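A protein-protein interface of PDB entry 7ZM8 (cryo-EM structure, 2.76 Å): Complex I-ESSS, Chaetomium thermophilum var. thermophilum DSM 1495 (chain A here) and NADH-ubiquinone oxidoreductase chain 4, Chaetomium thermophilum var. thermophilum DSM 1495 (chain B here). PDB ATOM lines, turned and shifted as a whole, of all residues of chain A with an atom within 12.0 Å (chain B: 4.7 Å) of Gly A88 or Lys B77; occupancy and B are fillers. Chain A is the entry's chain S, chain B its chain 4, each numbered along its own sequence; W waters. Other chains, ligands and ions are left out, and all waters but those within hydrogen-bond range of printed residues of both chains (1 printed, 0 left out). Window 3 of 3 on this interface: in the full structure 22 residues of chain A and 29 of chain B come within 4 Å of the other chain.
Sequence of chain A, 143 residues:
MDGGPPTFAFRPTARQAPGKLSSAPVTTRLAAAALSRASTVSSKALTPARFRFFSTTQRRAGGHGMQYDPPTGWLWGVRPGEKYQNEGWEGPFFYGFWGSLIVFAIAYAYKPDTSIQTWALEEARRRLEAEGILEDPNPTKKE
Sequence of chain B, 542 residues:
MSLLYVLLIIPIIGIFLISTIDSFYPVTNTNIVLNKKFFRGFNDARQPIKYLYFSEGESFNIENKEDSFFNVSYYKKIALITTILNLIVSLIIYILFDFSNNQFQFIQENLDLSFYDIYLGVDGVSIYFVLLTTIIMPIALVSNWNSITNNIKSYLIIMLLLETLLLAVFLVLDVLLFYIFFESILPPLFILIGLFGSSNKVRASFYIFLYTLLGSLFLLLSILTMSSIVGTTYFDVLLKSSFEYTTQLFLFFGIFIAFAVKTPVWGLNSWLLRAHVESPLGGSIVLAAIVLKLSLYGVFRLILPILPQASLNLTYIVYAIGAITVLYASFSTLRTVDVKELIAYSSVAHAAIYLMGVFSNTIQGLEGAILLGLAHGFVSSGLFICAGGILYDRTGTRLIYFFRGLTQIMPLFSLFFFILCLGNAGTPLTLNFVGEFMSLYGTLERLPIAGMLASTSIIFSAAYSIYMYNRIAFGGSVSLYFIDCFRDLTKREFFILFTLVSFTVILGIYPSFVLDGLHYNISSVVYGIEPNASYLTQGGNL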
ATOM      1  N   TYR A  84       5.750   3.262  19.875  1.00  0.00           N
ATOM      2  CA  TYR A  84       5.863   3.323  18.426  1.00  0.00           C
ATOM      3  C   TYR A  84       4.481   3.334  17.798  1.00  0.00           C
ATOM      4  O   TYR A  84       3.637   2.492  18.112  1.00  0.00           O
ATOM      5  CB  TYR A  84       6.668   2.144  17.894  1.00  0.00           C
ATOM      6  CG  TYR A  84       6.750   2.117  16.391  1.00  0.00           C
ATOM      7  CD1 TYR A  84       7.604   2.965  15.718  1.00  0.00           C
ATOM      8  CD2 TYR A  84       5.973   1.245  15.644  1.00  0.00           C
ATOM      9  CE1 TYR A  84       7.687   2.953  14.350  1.00  0.00           C
ATOM     10  CE2 TYR A  84       6.048   1.228  14.270  1.00  0.00           C
ATOM     11  CZ  TYR A  84       6.911   2.089  13.630  1.00  0.00           C
ATOM     12  OH  TYR A  84       7.011   2.094  12.262  1.00  0.00           O
ATOM     13  N   GLN A  85       4.256   4.276  16.895  1.00  0.00           N
ATOM     14  CA  GLN A  85       2.972   4.407  16.228  1.00  0.00           C
ATOM     15  C   GLN A  85       3.052   3.705  14.881  1.00  0.00           C
ATOM     16  O   GLN A  85       3.866   4.073  14.029  1.00  0.00           O
ATOM     17  CB  GLN A  85       2.604   5.880  16.064  1.00  0.00           C
ATOM     18  CG  GLN A  85       2.422   6.647  17.381  1.00  0.00           C
ATOM     19  CD  GLN A  85       1.717   5.860  18.482  1.00  0.00           C
ATOM     20  OE1 GLN A  85       0.874   5.000  18.224  1.00  0.00           O
ATOM     21  NE2 GLN A  85       2.082   6.148  19.725  1.00  0.00           N
ATOM     22  N   ASN A  86       2.174   2.743  14.604  1.00  0.00           N
ATOM     23  CA  ASN A  86       2.277   1.994  13.318  1.00  0.00           C
ATOM     24  C   ASN A  86       1.898   2.887  12.132  1.00  0.00           C
ATOM     25  O   ASN A  86       0.724   3.270  12.040  1.00  0.00           O
ATOM     26  CB  ASN A  86       1.487   0.685  13.304  1.00  0.00           C
ATOM     27  CG  ASN A  86       2.298  -0.502  13.776  1.00  0.00           C
ATOM     28  OD1 ASN A  86       2.252  -1.568  13.168  1.00  0.00           O
ATOM     29  ND2 ASN A  86       3.046  -0.328  14.851  1.00  0.00           N
ATOM     30  N   GLU A  87       2.855   3.194  11.258  1.00  0.00           N
ATOM     31  CA  GLU A  87       2.637   4.052  10.057  1.00  0.00           C
ATOM     32  C   GLU A  87       1.710   3.418   9.009  1.00  0.00           C
ATOM     33  O   GLU A  87       1.005   4.180   8.336  1.00  0.00           O
ATOM     34  CB  GLU A  87       3.985   4.434   9.459  1.00  0.00           C
ATOM     35  CG  GLU A  87       4.866   5.158  10.452  1.00  0.00           C
ATOM     36  CD  GLU A  87       6.228   5.506   9.891  1.00  0.00           C
ATOM     37  OE1 GLU A  87       6.951   6.283  10.543  1.00  0.00           O
ATOM     38  OE2 GLU A  87       6.558   4.994   8.805  1.00  0.00           O
ATOM     39  N   GLY A  88       1.774   2.100   8.803  1.00  0.00           N
ATOM     40  CA  GLY A  88       0.856   1.433   7.860  1.00  0.00           C
ATOM     41  C   GLY A  88       1.546   0.317   7.108  1.00  0.00           C
ATOM     42  O   GLY A  88       0.914  -0.737   6.924  1.00  0.00           O
ATOM     43  N   TRP A  89       2.789   0.546   6.678  1.00  0.00           N
ATOM     44  CA  TRP A  89       3.577  -0.475   5.995  1.00  0.00           C
ATOM     45  C   TRP A  89       3.837  -1.728   6.823  1.00  0.00           C
ATOM     46  O   TRP A  89       4.081  -2.787   6.243  1.00  0.00           O
ATOM     47  CB  TRP A  89       4.912   0.123   5.553  1.00  0.00           C
ATOM     48  CG  TRP A  89       5.774   0.528   6.703  1.00  0.00           C
ATOM     49  CD1 TRP A  89       5.806   1.740   7.308  1.00  0.00           C
ATOM     50  CD2 TRP A  89       6.726  -0.287   7.390  1.00  0.00           C
ATOM     51  NE1 TRP A  89       6.716   1.735   8.331  1.00  0.00           N
ATOM     52  CE2 TRP A  89       7.295   0.497   8.401  1.00  0.00           C
ATOM     53  CE3 TRP A  89       7.155  -1.607   7.245  1.00  0.00           C
ATOM     54  CZ2 TRP A  89       8.260   0.008   9.268  1.00  0.00           C
ATOM     55  CZ3 TRP A  89       8.108  -2.087   8.102  1.00  0.00           C
ATOM     56  CH2 TRP A  89       8.655  -1.282   9.099  1.00  0.00           C
ATOM     57  N   GLU A  90       3.790  -1.638   8.154  1.00  0.00           N
ATOM     58  CA  GLU A  90       4.337  -2.700   8.999  1.00  0.00           C
ATOM     59  C   GLU A  90       3.606  -4.023   8.808  1.00  0.00           C
ATOM     60  O   GLU A  90       4.237  -5.084   8.772  1.00  0.00           O
ATOM     61  CB  GLU A  90       4.287  -2.277  10.464  1.00  0.00           C
ATOM     62  CG  GLU A  90       5.265  -1.199  10.838  1.00  0.00           C
ATOM     63  CD  GLU A  90       4.705   0.186  10.635  1.00  0.00           C
ATOM     64  OE1 GLU A  90       3.757   0.324   9.851  1.00  0.00           O
ATOM     65  OE2 GLU A  90       5.213   1.138  11.252  1.00  0.00           O
ATOM     66  N   GLY A  91       2.283  -3.985   8.709  1.00  0.00           N
ATOM     67  CA  GLY A  91       1.486  -5.180   8.579  1.00  0.00           C
ATOM     68  C   GLY A  91       1.886  -6.062   7.416  1.00  0.00           C
ATOM     69  O   GLY A  91       2.336  -7.195   7.596  1.00  0.00           O
ATOM     70  N   PRO A  92       1.708  -5.566   6.191  1.00  0.00           N
ATOM     71  CA  PRO A  92       2.085  -6.370   5.021  1.00  0.00           C
ATOM     72  C   PRO A  92       3.562  -6.719   4.957  1.00  0.00           C
ATOM     73  O   PRO A  92       3.909  -7.813   4.501  1.00  0.00           O
ATOM     74  CB  PRO A  92       1.667  -5.482   3.842  1.00  0.00           C
ATOM     75  CG  PRO A  92       0.695  -4.520   4.400  1.00  0.00           C
ATOM     76  CD  PRO A  92       1.105  -4.281   5.804  1.00  0.00           C
ATOM     77  N   PHE A  93       4.447  -5.825   5.395  1.00  0.00           N
ATOM     78  CA  PHE A  93       5.875  -6.065   5.224  1.00  0.00           C
ATOM     79  C   PHE A  93       6.396  -7.135   6.172  1.00  0.00           C
ATOM     80  O   PHE A  93       7.328  -7.867   5.823  1.00  0.00           O
ATOM     81  CB  PHE A  93       6.641  -4.760   5.407  1.00  0.00           C
ATOM     82  CG  PHE A  93       8.096  -4.854   5.054  1.00  0.00           C
ATOM     83  CD1 PHE A  93       8.515  -4.690   3.748  1.00  0.00           C
ATOM     84  CD2 PHE A  93       9.048  -5.064   6.030  1.00  0.00           C
ATOM     85  CE1 PHE A  93       9.848  -4.761   3.425  1.00  0.00           C
ATOM     86  CE2 PHE A  93      10.377  -5.139   5.711  1.00  0.00           C
ATOM     87  CZ  PHE A  93      10.778  -4.982   4.411  1.00  0.00           C
ATOM     88  N   PHE A  94       5.830  -7.241   7.368  1.00  0.00           N
ATOM     89  CA  PHE A  94       6.285  -8.261   8.302  1.00  0.00           C
ATOM     90  C   PHE A  94       5.606  -9.600   8.065  1.00  0.00           C
ATOM     91  O   PHE A  94       6.246 -10.647   8.185  1.00  0.00           O
ATOM     92  CB  PHE A  94       6.052  -7.800   9.740  1.00  0.00           C
ATOM     93  CG  PHE A  94       6.961  -6.693  10.168  1.00  0.00           C
ATOM     94  CD1 PHE A  94       8.238  -6.599   9.660  1.00  0.00           C
ATOM     95  CD2 PHE A  94       6.534  -5.740  11.069  1.00  0.00           C
ATOM     96  CE1 PHE A  94       9.071  -5.581  10.047  1.00  0.00           C
ATOM     97  CE2 PHE A  94       7.370  -4.722  11.460  1.00  0.00           C
ATOM     98  CZ  PHE A  94       8.640  -4.645  10.948  1.00  0.00           C
ATOM     99  N   TYR A  95       4.326  -9.582   7.715  1.00  0.00           N
ATOM    100  CA  TYR A  95       3.566 -10.805   7.492  1.00  0.00           C
ATOM    101  C   TYR A  95       3.669 -11.302   6.060  1.00  0.00           C
ATOM    102  O   TYR A  95       3.808 -12.507   5.834  1.00  0.00           O
ATOM    103  CB  TYR A  95       2.099 -10.574   7.850  1.00  0.00           C
ATOM    104  CG  TYR A  95       1.872 -10.322   9.311  1.00  0.00           C
ATOM    105  CD1 TYR A  95       2.564 -11.040  10.270  1.00  0.00           C
ATOM    106  CD2 TYR A  95       0.971  -9.363   9.734  1.00  0.00           C
ATOM    107  CE1 TYR A  95       2.360 -10.813  11.612  1.00  0.00           C
ATOM    108  CE2 TYR A  95       0.758  -9.128  11.074  1.00  0.00           C
ATOM    109  CZ  TYR A  95       1.457  -9.857  12.009  1.00  0.00           C
ATOM    110  OH  TYR A  95       1.251  -9.627  13.349  1.00  0.00           O
ATOM    111  N   GLY A  96       3.604 -10.403   5.089  1.00  0.00           N
ATOM    112  CA  GLY A  96       3.588 -10.819   3.706  1.00  0.00           C
ATOM    113  C   GLY A  96       4.963 -10.908   3.090  1.00  0.00           C
ATOM    114  O   GLY A  96       5.313 -11.931   2.503  1.00  0.00           O
ATOM    115  N   PHE A  97       5.750  -9.841   3.208  1.00  0.00           N
ATOM    116  CA  PHE A  97       7.069  -9.836   2.589  1.00  0.00           C
ATOM    117  C   PHE A  97       7.997 -10.819   3.286  1.00  0.00           C
ATOM    118  O   PHE A  97       8.522 -11.742   2.660  1.00  0.00           O
ATOM    119  CB  PHE A  97       7.658  -8.428   2.596  1.00  0.00           C
ATOM    120  CG  PHE A  97       8.978  -8.328   1.894  1.00  0.00           C
ATOM    121  CD1 PHE A  97       9.036  -8.183   0.522  1.00  0.00           C
ATOM    122  CD2 PHE A  97      10.161  -8.389   2.606  1.00  0.00           C
ATOM    123  CE1 PHE A  97      10.246  -8.095  -0.123  1.00  0.00           C
ATOM    124  CE2 PHE A  97      11.369  -8.307   1.965  1.00  0.00           C
ATOM    125  CZ  PHE A  97      11.414  -8.163   0.600  1.00  0.00           C
ATOM    126  N   SER B  73      -3.405   6.687   3.047  1.00  0.00           N
ATOM    127  CA  SER B  73      -2.861   5.485   3.661  1.00  0.00           C
ATOM    128  C   SER B  73      -3.528   4.238   3.110  1.00  0.00           C
ATOM    129  O   SER B  73      -2.898   3.180   3.034  1.00  0.00           O
ATOM    130  CB  SER B  73      -3.028   5.547   5.177  1.00  0.00           C
ATOM    131  OG  SER B  73      -4.382   5.359   5.542  1.00  0.00           O
ATOM    132  N   TYR B  74      -4.782   4.342   2.699  1.00  0.00           N
ATOM    133  CA  TYR B  74      -5.506   3.186   2.122  1.00  0.00           C
ATOM    134  C   TYR B  74      -4.999   2.905   0.704  1.00  0.00           C
ATOM    135  O   TYR B  74      -4.891   1.735   0.339  1.00  0.00           O
ATOM    136  CB  TYR B  74      -6.996   3.514   2.123  1.00  0.00           C
ATOM    137  CG  TYR B  74      -7.927   2.348   2.339  1.00  0.00           C
ATOM    138  CD1 TYR B  74      -8.454   1.645   1.270  1.00  0.00           C
ATOM    139  CD2 TYR B  74      -8.306   1.965   3.614  1.00  0.00           C
ATOM    140  CE1 TYR B  74      -9.319   0.582   1.457  1.00  0.00           C
ATOM    141  CE2 TYR B  74      -9.172   0.904   3.820  1.00  0.00           C
ATOM    142  CZ  TYR B  74      -9.681   0.210   2.739  1.00  0.00           C
ATOM    143  OH  TYR B  74     -10.534  -0.838   2.931  1.00  0.00           O
ATOM    144  N   TYR B  75      -4.631   3.939  -0.039  1.00  0.00           N
ATOM    145  CA  TYR B  75      -4.079   3.795  -1.403  1.00  0.00           C
ATOM    146  C   TYR B  75      -2.729   3.111  -1.303  1.00  0.00           C
ATOM    147  O   TYR B  75      -2.367   2.351  -2.212  1.00  0.00           O
ATOM    148  CB  TYR B  75      -3.837   5.168  -2.025  1.00  0.00           C
ATOM    149  CG  TYR B  75      -5.049   5.988  -2.376  1.00  0.00           C
ATOM    150  CD1 TYR B  75      -6.088   5.456  -3.113  1.00  0.00           C
ATOM    151  CD2 TYR B  75      -5.128   7.318  -2.008  1.00  0.00           C
ATOM    152  CE1 TYR B  75      -7.200   6.216  -3.436  1.00  0.00           C
ATOM    153  CE2 TYR B  75      -6.229   8.092  -2.323  1.00  0.00           C
ATOM    154  CZ  TYR B  75      -7.272   7.537  -3.039  1.00  0.00           C
ATOM    155  OH  TYR B  75      -8.357   8.293  -3.367  1.00  0.00           O
ATOM    156  N   LYS B  76      -1.988   3.411  -0.240  1.00  0.00           N
ATOM    157  CA  LYS B  76      -0.599   2.919  -0.103  1.00  0.00           C
ATOM    158  C   LYS B  76      -0.549   1.495   0.428  1.00  0.00           C
ATOM    159  O   LYS B  76       0.465   0.843   0.200  1.00  0.00           O
ATOM    160  CB  LYS B  76       0.145   3.862   0.842  1.00  0.00           C
ATOM    161  CG  LYS B  76       0.987   4.938   0.182  1.00  0.00           C
ATOM    162  CD  LYS B  76       1.670   5.832   1.190  1.00  0.00           C
ATOM    163  CE  LYS B  76       0.686   6.640   2.004  1.00  0.00           C
ATOM    164  NZ  LYS B  76       1.327   7.243   3.192  1.00  0.00           N
ATOM    165  N   LYS B  77      -1.586   1.052   1.143  1.00  0.00           N
ATOM    166  CA  LYS B  77      -1.654  -0.349   1.533  1.00  0.00           C
ATOM    167  C   LYS B  77      -2.062  -1.226   0.362  1.00  0.00           C
ATOM    168  O   LYS B  77      -1.599  -2.363   0.247  1.00  0.00           O
ATOM    169  CB  LYS B  77      -2.617  -0.528   2.703  1.00  0.00           C
ATOM    170  CG  LYS B  77      -2.173   0.120   3.991  1.00  0.00           C
ATOM    171  CD  LYS B  77      -3.191  -0.135   5.087  1.00  0.00           C
ATOM    172  CE  LYS B  77      -2.742   0.421   6.429  1.00  0.00           C
ATOM    173  NZ  LYS B  77      -2.677   1.904   6.438  1.00  0.00           N
ATOM    174  N   ILE B  78      -2.929  -0.718  -0.514  1.00  0.00           N
ATOM    175  CA  ILE B  78      -3.326  -1.483  -1.691  1.00  0.00           C
ATOM    176  C   ILE B  78      -2.123  -1.737  -2.582  1.00  0.00           C
ATOM    177  O   ILE B  78      -1.895  -2.861  -3.044  1.00  0.00           O
ATOM    178  CB  ILE B  78      -4.444  -0.761  -2.459  1.00  0.00           C
ATOM    179  CG1 ILE B  78      -5.709  -0.666  -1.618  1.00  0.00           C
ATOM    180  CG2 ILE B  78      -4.739  -1.473  -3.769  1.00  0.00           C
ATOM    181  CD1 ILE B  78      -6.749   0.204  -2.235  1.00  0.00           C
ATOM    182  N   ALA B  79      -1.323  -0.700  -2.824  1.00  0.00           N
ATOM    183  CA  ALA B  79      -0.176  -0.843  -3.711  1.00  0.00           C
ATOM    184  C   ALA B  79       0.874  -1.771  -3.114  1.00  0.00           C
ATOM    185  O   ALA B  79       1.549  -2.508  -3.840  1.00  0.00           O
ATOM    186  CB  ALA B  79       0.422   0.528  -4.021  1.00  0.00           C
ATOM    187  N   LEU B  80       1.033  -1.746  -1.793  1.00  0.00           N
ATOM    188  CA  LEU B  80       2.038  -2.585  -1.156  1.00  0.00           C
ATOM    189  C   LEU B  80       1.598  -4.040  -1.074  1.00  0.00           C
ATOM    190  O   LEU B  80       2.411  -4.945  -1.281  1.00  0.00           O
ATOM    191  CB  LEU B  80       2.358  -2.051   0.235  1.00  0.00           C
ATOM    192  CG  LEU B  80       3.444  -2.805   0.988  1.00  0.00           C
ATOM    193  CD1 LEU B  80       4.760  -2.710   0.243  1.00  0.00           C
ATOM    194  CD2 LEU B  80       3.565  -2.264   2.388  1.00  0.00           C
ATOM    195  N   ILE B  81       0.333  -4.287  -0.736  1.00  0.00           N
ATOM    196  CA  ILE B  81      -0.182  -5.689  -0.693  1.00  0.00           C
ATOM    197  C   ILE B  81      -0.121  -6.279  -2.106  1.00  0.00           C
ATOM    198  O   ILE B  81       0.240  -7.460  -2.232  1.00  0.00           O
ATOM    199  CB  ILE B  81      -1.589  -5.765  -0.064  1.00  0.00           C
ATOM    200  CG1 ILE B  81      -1.566  -5.377   1.416  1.00  0.00           C
ATOM    201  CG2 ILE B  81      -2.213  -7.136  -0.263  1.00  0.00           C
ATOM    202  CD1 ILE B  81      -2.934  -5.327   2.051  1.00  0.00           C
ATOM    203  N   TRP B 145       7.685   5.855   1.347  1.00  0.00           N
ATOM    204  CA  TRP B 145       6.340   5.771   1.913  1.00  0.00           C
ATOM    205  C   TRP B 145       5.845   7.118   2.413  1.00  0.00           C
ATOM    206  O   TRP B 145       4.648   7.416   2.327  1.00  0.00           O
ATOM    207  CB  TRP B 145       6.336   4.747   3.047  1.00  0.00           C
ATOM    208  CG  TRP B 145       5.001   4.476   3.675  1.00  0.00           C
ATOM    209  CD1 TRP B 145       4.440   5.144   4.720  1.00  0.00           C
ATOM    210  CD2 TRP B 145       4.083   3.433   3.332  1.00  0.00           C
ATOM    211  NE1 TRP B 145       3.223   4.601   5.032  1.00  0.00           N
ATOM    212  CE2 TRP B 145       2.981   3.549   4.193  1.00  0.00           C
ATOM    213  CE3 TRP B 145       4.082   2.422   2.371  1.00  0.00           C
ATOM    214  CZ2 TRP B 145       1.893   2.694   4.126  1.00  0.00           C
ATOM    215  CZ3 TRP B 145       3.002   1.579   2.306  1.00  0.00           C
ATOM    216  CH2 TRP B 145       1.924   1.714   3.179  1.00  0.00           C
HETATM  217  O   HOH W   1      -1.508   3.877   8.307  1.00  0.00           O
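Of the 10 printed residues of chain B, 4 touch a printed residue of chain A.
Hydrophobic or aromatic side chains of chain A that line the printed part of chain B: Pro A92.
Gly A88 touches just these residues of chain B: Lys B77 and Trp B145.
Of chain A, only Gly A88 (3.8 Å) comes within 4 Å of Lys B77.
No residue of chain A comes within 4 Å of Tyr B74.
Lys B76 touches none of the printed residues of chain A.
No residue of chain A comes within 4 Å of Ile B78.
No residue of chain A comes within 4 Å of Ala B79.
Of the printed residues of chain A, Ile B81 touches Pro A92 (3.8 Å).
Printed residues of chain A within 4 Å of Leu B80: Trp A89 (3.9 Å).
Printed residues of chain B within 4 Å of Pro A92: Ile B81 (3.8 Å).
Of the printed residues of chain A, Trp B145 touches Gly A88 (3.8 Å) and Trp A89 (3.5 Å).
Glu A87 touches none of the printed residues of chain B.
Phe A93 touches none of the printed residues of chain B.
The nearest residue of chain A that does not touch Lys B77 is Glu A87 (4.7 Å).
The nearest printed residue of chain B that does not touch Pro A92 is Leu B80 (4.01 Å).
Among the printed residues, merely in contact across the chains: Trp A89 with Trp B145 (3.5 Å), Gly A88 with Trp B145 (3.8 Å), Gly A88 with Lys B77 (3.8 Å), Pro A92 with Ile B81 (3.8 Å) and Trp A89 with Leu B80 (3.9 Å).
OE2 of Glu A87 is in hydrogen-bond range of NE1 of Trp A89.
N of Gly A88 is in hydrogen-bond range of OE1 of Glu A90 (2.9 Å).
The indole nitrogen of Trp A89 sits at hydrogen-bond distance from the side-chain carboxylate of Glu A90 (3.3 Å).
The backbone NH (N) of Phe A97 lies within hydrogen-bond range of the backbone carbonyl oxygen (O) of Pro A92, at 3.0 Å.
O of Trp B145 is in hydrogen-bond range of NZ of Lys B76 (3.4 Å).
Water W1 lies within hydrogen-bond range of the backbone carbonyl oxygen (O) of Glu A87 and the side-chain amino group (NZ) of Lys B77.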
